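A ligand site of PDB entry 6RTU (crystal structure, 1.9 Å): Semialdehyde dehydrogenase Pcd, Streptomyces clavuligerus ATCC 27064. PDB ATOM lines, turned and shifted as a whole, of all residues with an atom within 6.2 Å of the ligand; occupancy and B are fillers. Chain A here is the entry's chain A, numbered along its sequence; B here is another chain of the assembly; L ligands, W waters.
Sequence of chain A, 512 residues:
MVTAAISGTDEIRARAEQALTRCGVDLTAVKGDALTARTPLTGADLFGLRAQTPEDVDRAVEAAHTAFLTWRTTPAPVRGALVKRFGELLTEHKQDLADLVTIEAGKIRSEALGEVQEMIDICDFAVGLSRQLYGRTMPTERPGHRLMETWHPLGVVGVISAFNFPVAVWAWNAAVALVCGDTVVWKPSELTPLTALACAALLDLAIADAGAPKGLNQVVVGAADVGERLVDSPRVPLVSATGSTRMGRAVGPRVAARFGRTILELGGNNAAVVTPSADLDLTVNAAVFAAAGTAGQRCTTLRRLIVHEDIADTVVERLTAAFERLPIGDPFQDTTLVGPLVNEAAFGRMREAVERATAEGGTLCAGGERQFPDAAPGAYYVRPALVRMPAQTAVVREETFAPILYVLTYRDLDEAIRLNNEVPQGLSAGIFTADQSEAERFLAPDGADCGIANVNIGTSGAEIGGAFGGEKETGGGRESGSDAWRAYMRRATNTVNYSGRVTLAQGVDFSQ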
ATOM      1  N   GLU A 118     -28.292  22.310 -17.120  1.00  0.00           N
ATOM      2  CA  GLU A 118     -27.585  21.030 -17.114  1.00  0.00           C
ATOM      3  C   GLU A 118     -26.393  21.081 -16.152  1.00  0.00           C
ATOM      4  O   GLU A 118     -26.151  20.118 -15.413  1.00  0.00           O
ATOM      5  CB  GLU A 118     -27.112  20.661 -18.517  1.00  0.00           C
ATOM      6  CG  GLU A 118     -28.192  20.252 -19.528  1.00  0.00           C
ATOM      7  CD  GLU A 118     -27.593  19.615 -20.765  1.00  0.00           C
ATOM      8  OE1 GLU A 118     -27.841  20.135 -21.890  1.00  0.00           O
ATOM      9  OE2 GLU A 118     -26.856  18.615 -20.614  1.00  0.00           O
ATOM     10  N   ASN A 164     -20.738  24.189 -29.668  1.00  0.00           N
ATOM     11  CA  ASN A 164     -22.198  24.099 -29.665  1.00  0.00           C
ATOM     12  C   ASN A 164     -22.765  23.835 -28.282  1.00  0.00           C
ATOM     13  O   ASN A 164     -23.919  24.204 -28.009  1.00  0.00           O
ATOM     14  CB  ASN A 164     -22.659  23.026 -30.661  1.00  0.00           C
ATOM     15  CG  ASN A 164     -22.095  21.639 -30.373  1.00  0.00           C
ATOM     16  OD1 ASN A 164     -20.997  21.491 -29.831  1.00  0.00           O
ATOM     17  ND2 ASN A 164     -22.847  20.607 -30.749  1.00  0.00           N
ATOM     18  N   PHE A 165     -21.995  23.223 -27.375  1.00  0.00           N
ATOM     19  CA  PHE A 165     -22.342  23.180 -25.948  1.00  0.00           C
ATOM     20  C   PHE A 165     -21.156  23.709 -25.161  1.00  0.00           C
ATOM     21  O   PHE A 165     -20.348  22.941 -24.608  1.00  0.00           O
ATOM     22  CB  PHE A 165     -22.755  21.768 -25.521  1.00  0.00           C
ATOM     23  CG  PHE A 165     -24.165  21.469 -25.863  1.00  0.00           C
ATOM     24  CD1 PHE A 165     -24.492  21.034 -27.134  1.00  0.00           C
ATOM     25  CD2 PHE A 165     -25.180  21.686 -24.945  1.00  0.00           C
ATOM     26  CE1 PHE A 165     -25.812  20.784 -27.469  1.00  0.00           C
ATOM     27  CE2 PHE A 165     -26.496  21.434 -25.270  1.00  0.00           C
ATOM     28  CZ  PHE A 165     -26.813  20.992 -26.546  1.00  0.00           C
ATOM     29  N   VAL A 169     -20.889  20.609 -21.464  1.00  0.00           N
ATOM     30  CA  VAL A 169     -19.965  19.489 -21.618  1.00  0.00           C
ATOM     31  C   VAL A 169     -18.844  19.580 -20.590  1.00  0.00           C
ATOM     32  O   VAL A 169     -18.527  18.603 -19.893  1.00  0.00           O
ATOM     33  CB  VAL A 169     -19.429  19.403 -23.061  1.00  0.00           C
ATOM     34  CG1 VAL A 169     -18.212  18.482 -23.127  1.00  0.00           C
ATOM     35  CG2 VAL A 169     -20.520  18.905 -23.996  1.00  0.00           C
ATOM     36  N   TRP A 172     -20.249  18.592 -17.156  1.00  0.00           N
ATOM     37  CA  TRP A 172     -20.334  17.148 -16.984  1.00  0.00           C
ATOM     38  C   TRP A 172     -18.999  16.583 -16.536  1.00  0.00           C
ATOM     39  O   TRP A 172     -18.925  15.768 -15.614  1.00  0.00           O
ATOM     40  CB  TRP A 172     -20.712  16.424 -18.276  1.00  0.00           C
ATOM     41  CG  TRP A 172     -22.007  16.763 -18.950  1.00  0.00           C
ATOM     42  CD1 TRP A 172     -23.086  17.359 -18.396  1.00  0.00           C
ATOM     43  CD2 TRP A 172     -22.339  16.481 -20.311  1.00  0.00           C
ATOM     44  NE1 TRP A 172     -24.076  17.512 -19.344  1.00  0.00           N
ATOM     45  CE2 TRP A 172     -23.641  16.980 -20.535  1.00  0.00           C
ATOM     46  CE3 TRP A 172     -21.653  15.901 -21.387  1.00  0.00           C
ATOM     47  CZ2 TRP A 172     -24.295  16.882 -21.768  1.00  0.00           C
ATOM     48  CZ3 TRP A 172     -22.297  15.795 -22.625  1.00  0.00           C
ATOM     49  CH2 TRP A 172     -23.604  16.294 -22.803  1.00  0.00           C
ATOM     50  N   THR A 242     -15.405  15.969 -26.772  1.00  0.00           N
ATOM     51  CA  THR A 242     -16.795  15.945 -27.192  1.00  0.00           C
ATOM     52  C   THR A 242     -16.990  16.980 -28.292  1.00  0.00           C
ATOM     53  O   THR A 242     -16.560  18.128 -28.145  1.00  0.00           O
ATOM     54  CB  THR A 242     -17.750  16.263 -26.041  1.00  0.00           C
ATOM     55  OG1 THR A 242     -17.509  15.351 -24.960  1.00  0.00           O
ATOM     56  CG2 THR A 242     -19.217  16.126 -26.497  1.00  0.00           C
ATOM     57  N   GLY A 243     -17.654  16.580 -29.368  1.00  0.00           N
ATOM     58  CA  GLY A 243     -17.929  17.509 -30.446  1.00  0.00           C
ATOM     59  C   GLY A 243     -17.555  16.978 -31.819  1.00  0.00           C
ATOM     60  O   GLY A 243     -16.781  16.021 -31.944  1.00  0.00           O
ATOM     61  N   GLU A 265     -16.797  11.411 -27.873  1.00  0.00           N
ATOM     62  CA  GLU A 265     -18.144  11.535 -28.436  1.00  0.00           C
ATOM     63  C   GLU A 265     -17.997  12.500 -29.608  1.00  0.00           C
ATOM     64  O   GLU A 265     -17.933  13.722 -29.422  1.00  0.00           O
ATOM     65  CB  GLU A 265     -19.153  12.038 -27.406  1.00  0.00           C
ATOM     66  CG  GLU A 265     -20.627  11.941 -27.862  1.00  0.00           C
ATOM     67  CD  GLU A 265     -20.928  12.958 -28.937  1.00  0.00           C
ATOM     68  OE1 GLU A 265     -21.153  14.134 -28.587  1.00  0.00           O
ATOM     69  OE2 GLU A 265     -20.920  12.577 -30.138  1.00  0.00           O
ATOM     70  N   GLN A 297     -27.416  22.114 -34.853  1.00  0.00           N
ATOM     71  CA  GLN A 297     -25.993  22.018 -34.529  1.00  0.00           C
ATOM     72  C   GLN A 297     -25.747  21.272 -33.215  1.00  0.00           C
ATOM     73  O   GLN A 297     -24.866  21.627 -32.442  1.00  0.00           O
ATOM     74  CB  GLN A 297     -25.355  23.398 -34.495  1.00  0.00           C
ATOM     75  CG  GLN A 297     -25.442  24.166 -35.831  1.00  0.00           C
ATOM     76  CD  GLN A 297     -24.935  25.614 -35.704  1.00  0.00           C
ATOM     77  OE1 GLN A 297     -24.084  26.046 -36.472  1.00  0.00           O
ATOM     78  NE2 GLN A 297     -25.471  26.356 -34.732  1.00  0.00           N
ATOM     79  N   ARG A 298     -26.513  20.224 -32.941  1.00  0.00           N
ATOM     80  CA  ARG A 298     -26.197  19.301 -31.866  1.00  0.00           C
ATOM     81  C   ARG A 298     -25.621  18.016 -32.440  1.00  0.00           C
ATOM     82  O   ARG A 298     -25.972  17.606 -33.546  1.00  0.00           O
ATOM     83  CB  ARG A 298     -27.439  18.974 -31.023  1.00  0.00           C
ATOM     84  CG  ARG A 298     -28.237  20.158 -30.526  1.00  0.00           C
ATOM     85  CD  ARG A 298     -29.228  19.682 -29.434  1.00  0.00           C
ATOM     86  NE  ARG A 298     -29.956  20.760 -28.787  1.00  0.00           N
ATOM     87  CZ  ARG A 298     -30.580  20.647 -27.616  1.00  0.00           C
ATOM     88  NH1 ARG A 298     -30.583  19.487 -26.950  1.00  0.00           N
ATOM     89  NH2 ARG A 298     -31.206  21.692 -27.098  1.00  0.00           N
ATOM     90  N   CYS A 299     -24.741  17.355 -31.679  1.00  0.00           N
ATOM     91  CA  CYS A 299     -24.356  16.006 -32.095  1.00  0.00           C
ATOM     92  C   CYS A 299     -25.570  15.080 -32.099  1.00  0.00           C
ATOM     93  O   CYS A 299     -25.613  14.119 -32.874  1.00  0.00           O
ATOM     94  CB  CYS A 299     -23.244  15.462 -31.184  1.00  0.00           C
ATOM     95  SG  CYS A 299     -21.607  16.356 -31.341  1.00  0.00           S
ATOM     96  N   THR A 300     -26.575  15.393 -31.287  1.00  0.00           N
ATOM     97  CA  THR A 300     -27.804  14.613 -31.163  1.00  0.00           C
ATOM     98  C   THR A 300     -28.910  15.071 -32.102  1.00  0.00           C
ATOM     99  O   THR A 300     -30.044  14.571 -31.986  1.00  0.00           O
ATOM    100  CB  THR A 300     -28.321  14.693 -29.728  1.00  0.00           C
ATOM    101  OG1 THR A 300     -28.472  16.086 -29.391  1.00  0.00           O
ATOM    102  CG2 THR A 300     -27.330  14.042 -28.759  1.00  0.00           C
ATOM    103  N   THR A 301     -28.639  16.014 -33.011  1.00  0.00           N
ATOM    104  CA  THR A 301     -29.684  16.556 -33.882  1.00  0.00           C
ATOM    105  C   THR A 301     -30.316  15.454 -34.735  1.00  0.00           C
ATOM    106  O   THR A 301     -29.648  14.525 -35.194  1.00  0.00           O
ATOM    107  CB  THR A 301     -29.107  17.664 -34.779  1.00  0.00           C
ATOM    108  OG1 THR A 301     -28.916  18.844 -33.988  1.00  0.00           O
ATOM    109  CG2 THR A 301     -30.030  18.010 -35.966  1.00  0.00           C
ATOM    110  N   PHE A 401     -23.332  19.344 -40.350  1.00  0.00           N
ATOM    111  CA  PHE A 401     -23.654  20.037 -39.087  1.00  0.00           C
ATOM    112  C   PHE A 401     -24.491  21.268 -39.409  1.00  0.00           C
ATOM    113  O   PHE A 401     -24.059  22.420 -39.284  1.00  0.00           O
ATOM    114  CB  PHE A 401     -22.377  20.376 -38.322  1.00  0.00           C
ATOM    115  CG  PHE A 401     -22.452  20.090 -36.822  1.00  0.00           C
ATOM    116  CD1 PHE A 401     -22.625  18.789 -36.355  1.00  0.00           C
ATOM    117  CD2 PHE A 401     -22.314  21.120 -35.886  1.00  0.00           C
ATOM    118  CE1 PHE A 401     -22.679  18.512 -34.980  1.00  0.00           C
ATOM    119  CE2 PHE A 401     -22.372  20.854 -34.518  1.00  0.00           C
ATOM    120  CZ  PHE A 401     -22.549  19.554 -34.061  1.00  0.00           C
ATOM    121  N   LEU A 427     -24.977   7.517 -32.397  1.00  0.00           N
ATOM    122  CA  LEU A 427     -25.210   8.267 -31.157  1.00  0.00           C
ATOM    123  C   LEU A 427     -26.604   8.015 -30.601  1.00  0.00           C
ATOM    124  O   LEU A 427     -26.745   7.384 -29.546  1.00  0.00           O
ATOM    125  CB  LEU A 427     -24.933   9.762 -31.369  1.00  0.00           C
ATOM    126  CG  LEU A 427     -25.088  10.664 -30.132  1.00  0.00           C
ATOM    127  CD1 LEU A 427     -24.423  10.073 -28.891  1.00  0.00           C
ATOM    128  CD2 LEU A 427     -24.539  12.061 -30.417  1.00  0.00           C
ATOM    129  N   ILE A 452     -27.959   5.737 -27.461  1.00  0.00           N
ATOM    130  CA  ILE A 452     -29.226   6.247 -26.939  1.00  0.00           C
ATOM    131  C   ILE A 452     -30.334   5.788 -27.873  1.00  0.00           C
ATOM    132  O   ILE A 452     -30.221   5.967 -29.093  1.00  0.00           O
ATOM    133  CB  ILE A 452     -29.204   7.790 -26.833  1.00  0.00           C
ATOM    134  CG1 ILE A 452     -28.101   8.246 -25.887  1.00  0.00           C
ATOM    135  CG2 ILE A 452     -30.615   8.337 -26.468  1.00  0.00           C
ATOM    136  CD1 ILE A 452     -27.689   9.732 -26.086  1.00  0.00           C
ATOM    137  N   THR A 459     -34.267  12.473 -30.847  1.00  0.00           N
ATOM    138  CA  THR A 459     -32.887  12.061 -30.659  1.00  0.00           C
ATOM    139  C   THR A 459     -32.082  12.983 -29.739  1.00  0.00           C
ATOM    140  O   THR A 459     -31.003  12.577 -29.299  1.00  0.00           O
ATOM    141  CB  THR A 459     -32.193  11.965 -32.021  1.00  0.00           C
ATOM    142  OG1 THR A 459     -32.364  13.204 -32.717  1.00  0.00           O
ATOM    143  CG2 THR A 459     -32.783  10.824 -32.863  1.00  0.00           C
ATOM    144  N   SER A 460     -32.576  14.176 -29.417  1.00  0.00           N
ATOM    145  CA  SER A 460     -31.825  15.152 -28.630  1.00  0.00           C
ATOM    146  C   SER A 460     -32.490  15.384 -27.266  1.00  0.00           C
ATOM    147  O   SER A 460     -33.545  14.821 -26.953  1.00  0.00           O
ATOM    148  CB  SER A 460     -31.699  16.486 -29.376  1.00  0.00           C
ATOM    149  OG  SER A 460     -32.965  17.077 -29.574  1.00  0.00           O
ATOM    150  N   GLY A 461     -31.829  16.200 -26.452  1.00  0.00           N
ATOM    151  CA  GLY A 461     -32.388  16.619 -25.181  1.00  0.00           C
ATOM    152  C   GLY A 461     -32.315  15.596 -24.056  1.00  0.00           C
ATOM    153  O   GLY A 461     -33.269  15.458 -23.276  1.00  0.00           O
ATOM    154  N   ALA A 462     -31.195  14.883 -23.944  1.00  0.00           N
ATOM    155  CA  ALA A 462     -30.989  13.927 -22.867  1.00  0.00           C
ATOM    156  C   ALA A 462     -31.000  14.623 -21.502  1.00  0.00           C
ATOM    157  O   ALA A 462     -30.716  15.821 -21.379  1.00  0.00           O
ATOM    158  CB  ALA A 462     -29.655  13.198 -23.051  1.00  0.00           C
ATOM    159  N   GLU A 463     -31.303  13.855 -20.465  1.00  0.00           N
ATOM    160  CA  GLU A 463     -31.174  14.362 -19.108  1.00  0.00           C
ATOM    161  C   GLU A 463     -29.921  13.800 -18.425  1.00  0.00           C
ATOM    162  O   GLU A 463     -29.327  12.821 -18.876  1.00  0.00           O
ATOM    163  CB  GLU A 463     -32.427  14.077 -18.275  1.00  0.00           C
ATOM    164  CG  GLU A 463     -32.996  12.677 -18.371  1.00  0.00           C
ATOM    165  CD  GLU A 463     -34.332  12.567 -17.629  1.00  0.00           C
ATOM    166  OE1 GLU A 463     -34.277  12.504 -16.386  1.00  0.00           O
ATOM    167  OE2 GLU A 463     -35.433  12.568 -18.259  1.00  0.00           O
ATOM    168  N   ILE A 464     -29.552  14.427 -17.309  1.00  0.00           N
ATOM    169  CA  ILE A 464     -28.245  14.232 -16.679  1.00  0.00           C
ATOM    170  C   ILE A 464     -28.093  12.851 -16.055  1.00  0.00           C
ATOM    171  O   ILE A 464     -26.960  12.370 -15.907  1.00  0.00           O
ATOM    172  CB  ILE A 464     -28.014  15.378 -15.660  1.00  0.00           C
ATOM    173  CG1 ILE A 464     -27.012  16.378 -16.214  1.00  0.00           C
ATOM    174  CG2 ILE A 464     -27.698  14.863 -14.236  1.00  0.00           C
ATOM    175  CD1 ILE A 464     -27.426  16.942 -17.583  1.00  0.00           C
ATOM    176  N   PHE A 468     -24.330   9.322 -21.197  1.00  0.00           N
ATOM    177  CA  PHE A 468     -24.459   9.984 -22.493  1.00  0.00           C
ATOM    178  C   PHE A 468     -23.248   9.638 -23.376  1.00  0.00           C
ATOM    179  O   PHE A 468     -22.101   9.820 -22.957  1.00  0.00           O
ATOM    180  CB  PHE A 468     -24.574  11.500 -22.331  1.00  0.00           C
ATOM    181  CG  PHE A 468     -24.601  12.280 -23.644  1.00  0.00           C
ATOM    182  CD1 PHE A 468     -23.423  12.637 -24.275  1.00  0.00           C
ATOM    183  CD2 PHE A 468     -25.799  12.662 -24.227  1.00  0.00           C
ATOM    184  CE1 PHE A 468     -23.428  13.343 -25.468  1.00  0.00           C
ATOM    185  CE2 PHE A 468     -25.823  13.364 -25.415  1.00  0.00           C
ATOM    186  CZ  PHE A 468     -24.637  13.709 -26.029  1.00  0.00           C
ATOM    187  N   GLN B 506     -34.777  19.871 -18.844  1.00  0.00           N
ATOM    188  CA  GLN B 506     -34.178  21.135 -18.383  1.00  0.00           C
ATOM    189  C   GLN B 506     -35.087  22.342 -18.586  1.00  0.00           C
ATOM    190  O   GLN B 506     -34.594  23.480 -18.604  1.00  0.00           O
ATOM    191  CB  GLN B 506     -32.824  21.406 -19.050  1.00  0.00           C
ATOM    192  CG  GLN B 506     -31.730  20.431 -18.681  1.00  0.00           C
ATOM    193  CD  GLN B 506     -31.530  19.364 -19.748  1.00  0.00           C
ATOM    194  OE1 GLN B 506     -31.642  19.646 -20.943  1.00  0.00           O
ATOM    195  NE2 GLN B 506     -31.244  18.130 -19.310  1.00  0.00           N
HETATM  196  C1  LIG L   1     -23.685  17.613 -28.084  1.00  0.00           C
HETATM  197  O1  LIG L   1     -24.466  17.816 -29.056  1.00  0.00           O
HETATM  198  O2  LIG L   1     -22.443  17.653 -28.253  1.00  0.00           O
HETATM  199  O3  LIG L   1     -28.758  15.477 -25.418  1.00  0.00           O
HETATM  200  C2  LIG L   1     -24.240  17.297 -26.692  1.00  0.00           C
HETATM  201  C3  LIG L   1     -28.590  16.655 -25.839  1.00  0.00           C
HETATM  202  C4  LIG L   1     -27.772  17.663 -25.028  1.00  0.00           C
HETATM  203  C5  LIG L   1     -26.268  17.434 -25.199  1.00  0.00           C
HETATM  204  C6  LIG L   1     -25.774  17.300 -26.635  1.00  0.00           C
HETATM  205  N1  LIG L   1     -28.119  17.530 -23.617  1.00  0.00           N
HETATM  206  O4  LIG L   1     -29.122  17.033 -26.927  1.00  0.00           O
HETATM  207  O   HOH W   1     -30.193  12.867 -26.515  1.00  0.00           O
HETATM  208  O   HOH W   2     -20.682  19.484 -27.917  1.00  0.00           O
HETATM  209  O   HOH W   3     -27.475  15.896 -21.156  1.00  0.00           O
HETATM  210  O   HOH W   4     -30.779  18.051 -22.808  1.00  0.00           O
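Asn 164 touches the ligand (ND2 to O1, 3.6 Å). Phe 165 touches the ligand (CE1 to C6, 3.6 Å). Trp 172 touches the ligand. CG2 of Thr 242 touches O2 of the ligand (3.98 Å). Glu 265 touches the ligand. CB of Ser 460 touches O4 of the ligand (3.6 Å). CE2 of Phe 468 touches O3 of the ligand, at 3.6 Å. Hydrophobic or aromatic side chains that line the ligand: Phe 165, Trp 172, Ala 462 and Phe 468. Within 4 Å of the ligand: Glu 118, Asn 164, Phe 165, Trp 172, Thr 242, Glu 265, Arg 298, Cys 299, Thr 300, Ser 460, Gly 461, Ala 462 and Phe 468.
Water W2 lies within hydrogen-bond range of O2 of the ligand and OD1 of Asn 164. Water W4 lies within hydrogen-bond range of OE1 of Gln 506 of chain B (2.6 Å), O of Ala 462 (2.6 Å) and N1 of the ligand (2.8 Å). Water W3 lies within hydrogen-bond range of the side-chain carboxylate of Glu 118 (2.8 Å), a nitrogen (N1) of the ligand (3.0 Å) and the backbone carbonyl oxygen of Ala 462 (3.2 Å). Water W1 lies within hydrogen-bond range of O of Thr 459 (2.9 Å), O3 of the ligand (3.2 Å) and N of Ala 462 (3.4 Å).
SG of Cys 299 sits at hydrogen-bond distance from OE1 of Glu 265 (3.6 Å). The side-chain hydroxyl of Thr 459 lies within hydrogen-bond range of the backbone carbonyl oxygen of Thr 300 (2.8 Å). The side-chain hydroxyl (OG1) of Thr 301 lies within hydrogen-bond range of the backbone NH (N) of Arg 298. The backbone carbonyl oxygen of Ala 462 is in hydrogen-bond range of the side-chain amide nitrogen of Gln 506 of chain B (3.1 Å). The indole nitrogen (NE1) of Trp 172 is in hydrogen-bond range of the side-chain carboxylate (OE2) of Glu 118 (3.2 Å). The side-chain amide nitrogen of Asn 164 sits at hydrogen-bond distance from the backbone carbonyl oxygen of Gln 297. The backbone NH of Gly 243 is in hydrogen-bond range of the backbone carbonyl oxygen of Glu 265 (2.9 Å).
N of Cys 299 sits at hydrogen-bond distance from O1 of the ligand (2.7 Å). An oxygen (O2) of the ligand lies within hydrogen-bond range of the side-chain sulfur (SG) of Cys 299 (3.5 Å). OG1 of Thr 300 is in hydrogen-bond range of O4 of the ligand (2.7 Å). An oxygen (O4) of the ligand is in salt-bridge range of the guanidinium group (NH1) of Arg 298, at 2.9 Å. O4 of the ligand lies within hydrogen-bond range of N of Gly 461, at 2.9 Å. The backbone NH (N) of Ala 462 sits at hydrogen-bond distance from an oxygen (O3) of the ligand, at 2.9 Å. The side-chain carboxylate (OE1) of Glu 118 lies within salt-bridge range of a nitrogen (N1) of the ligand (3.1 Å).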
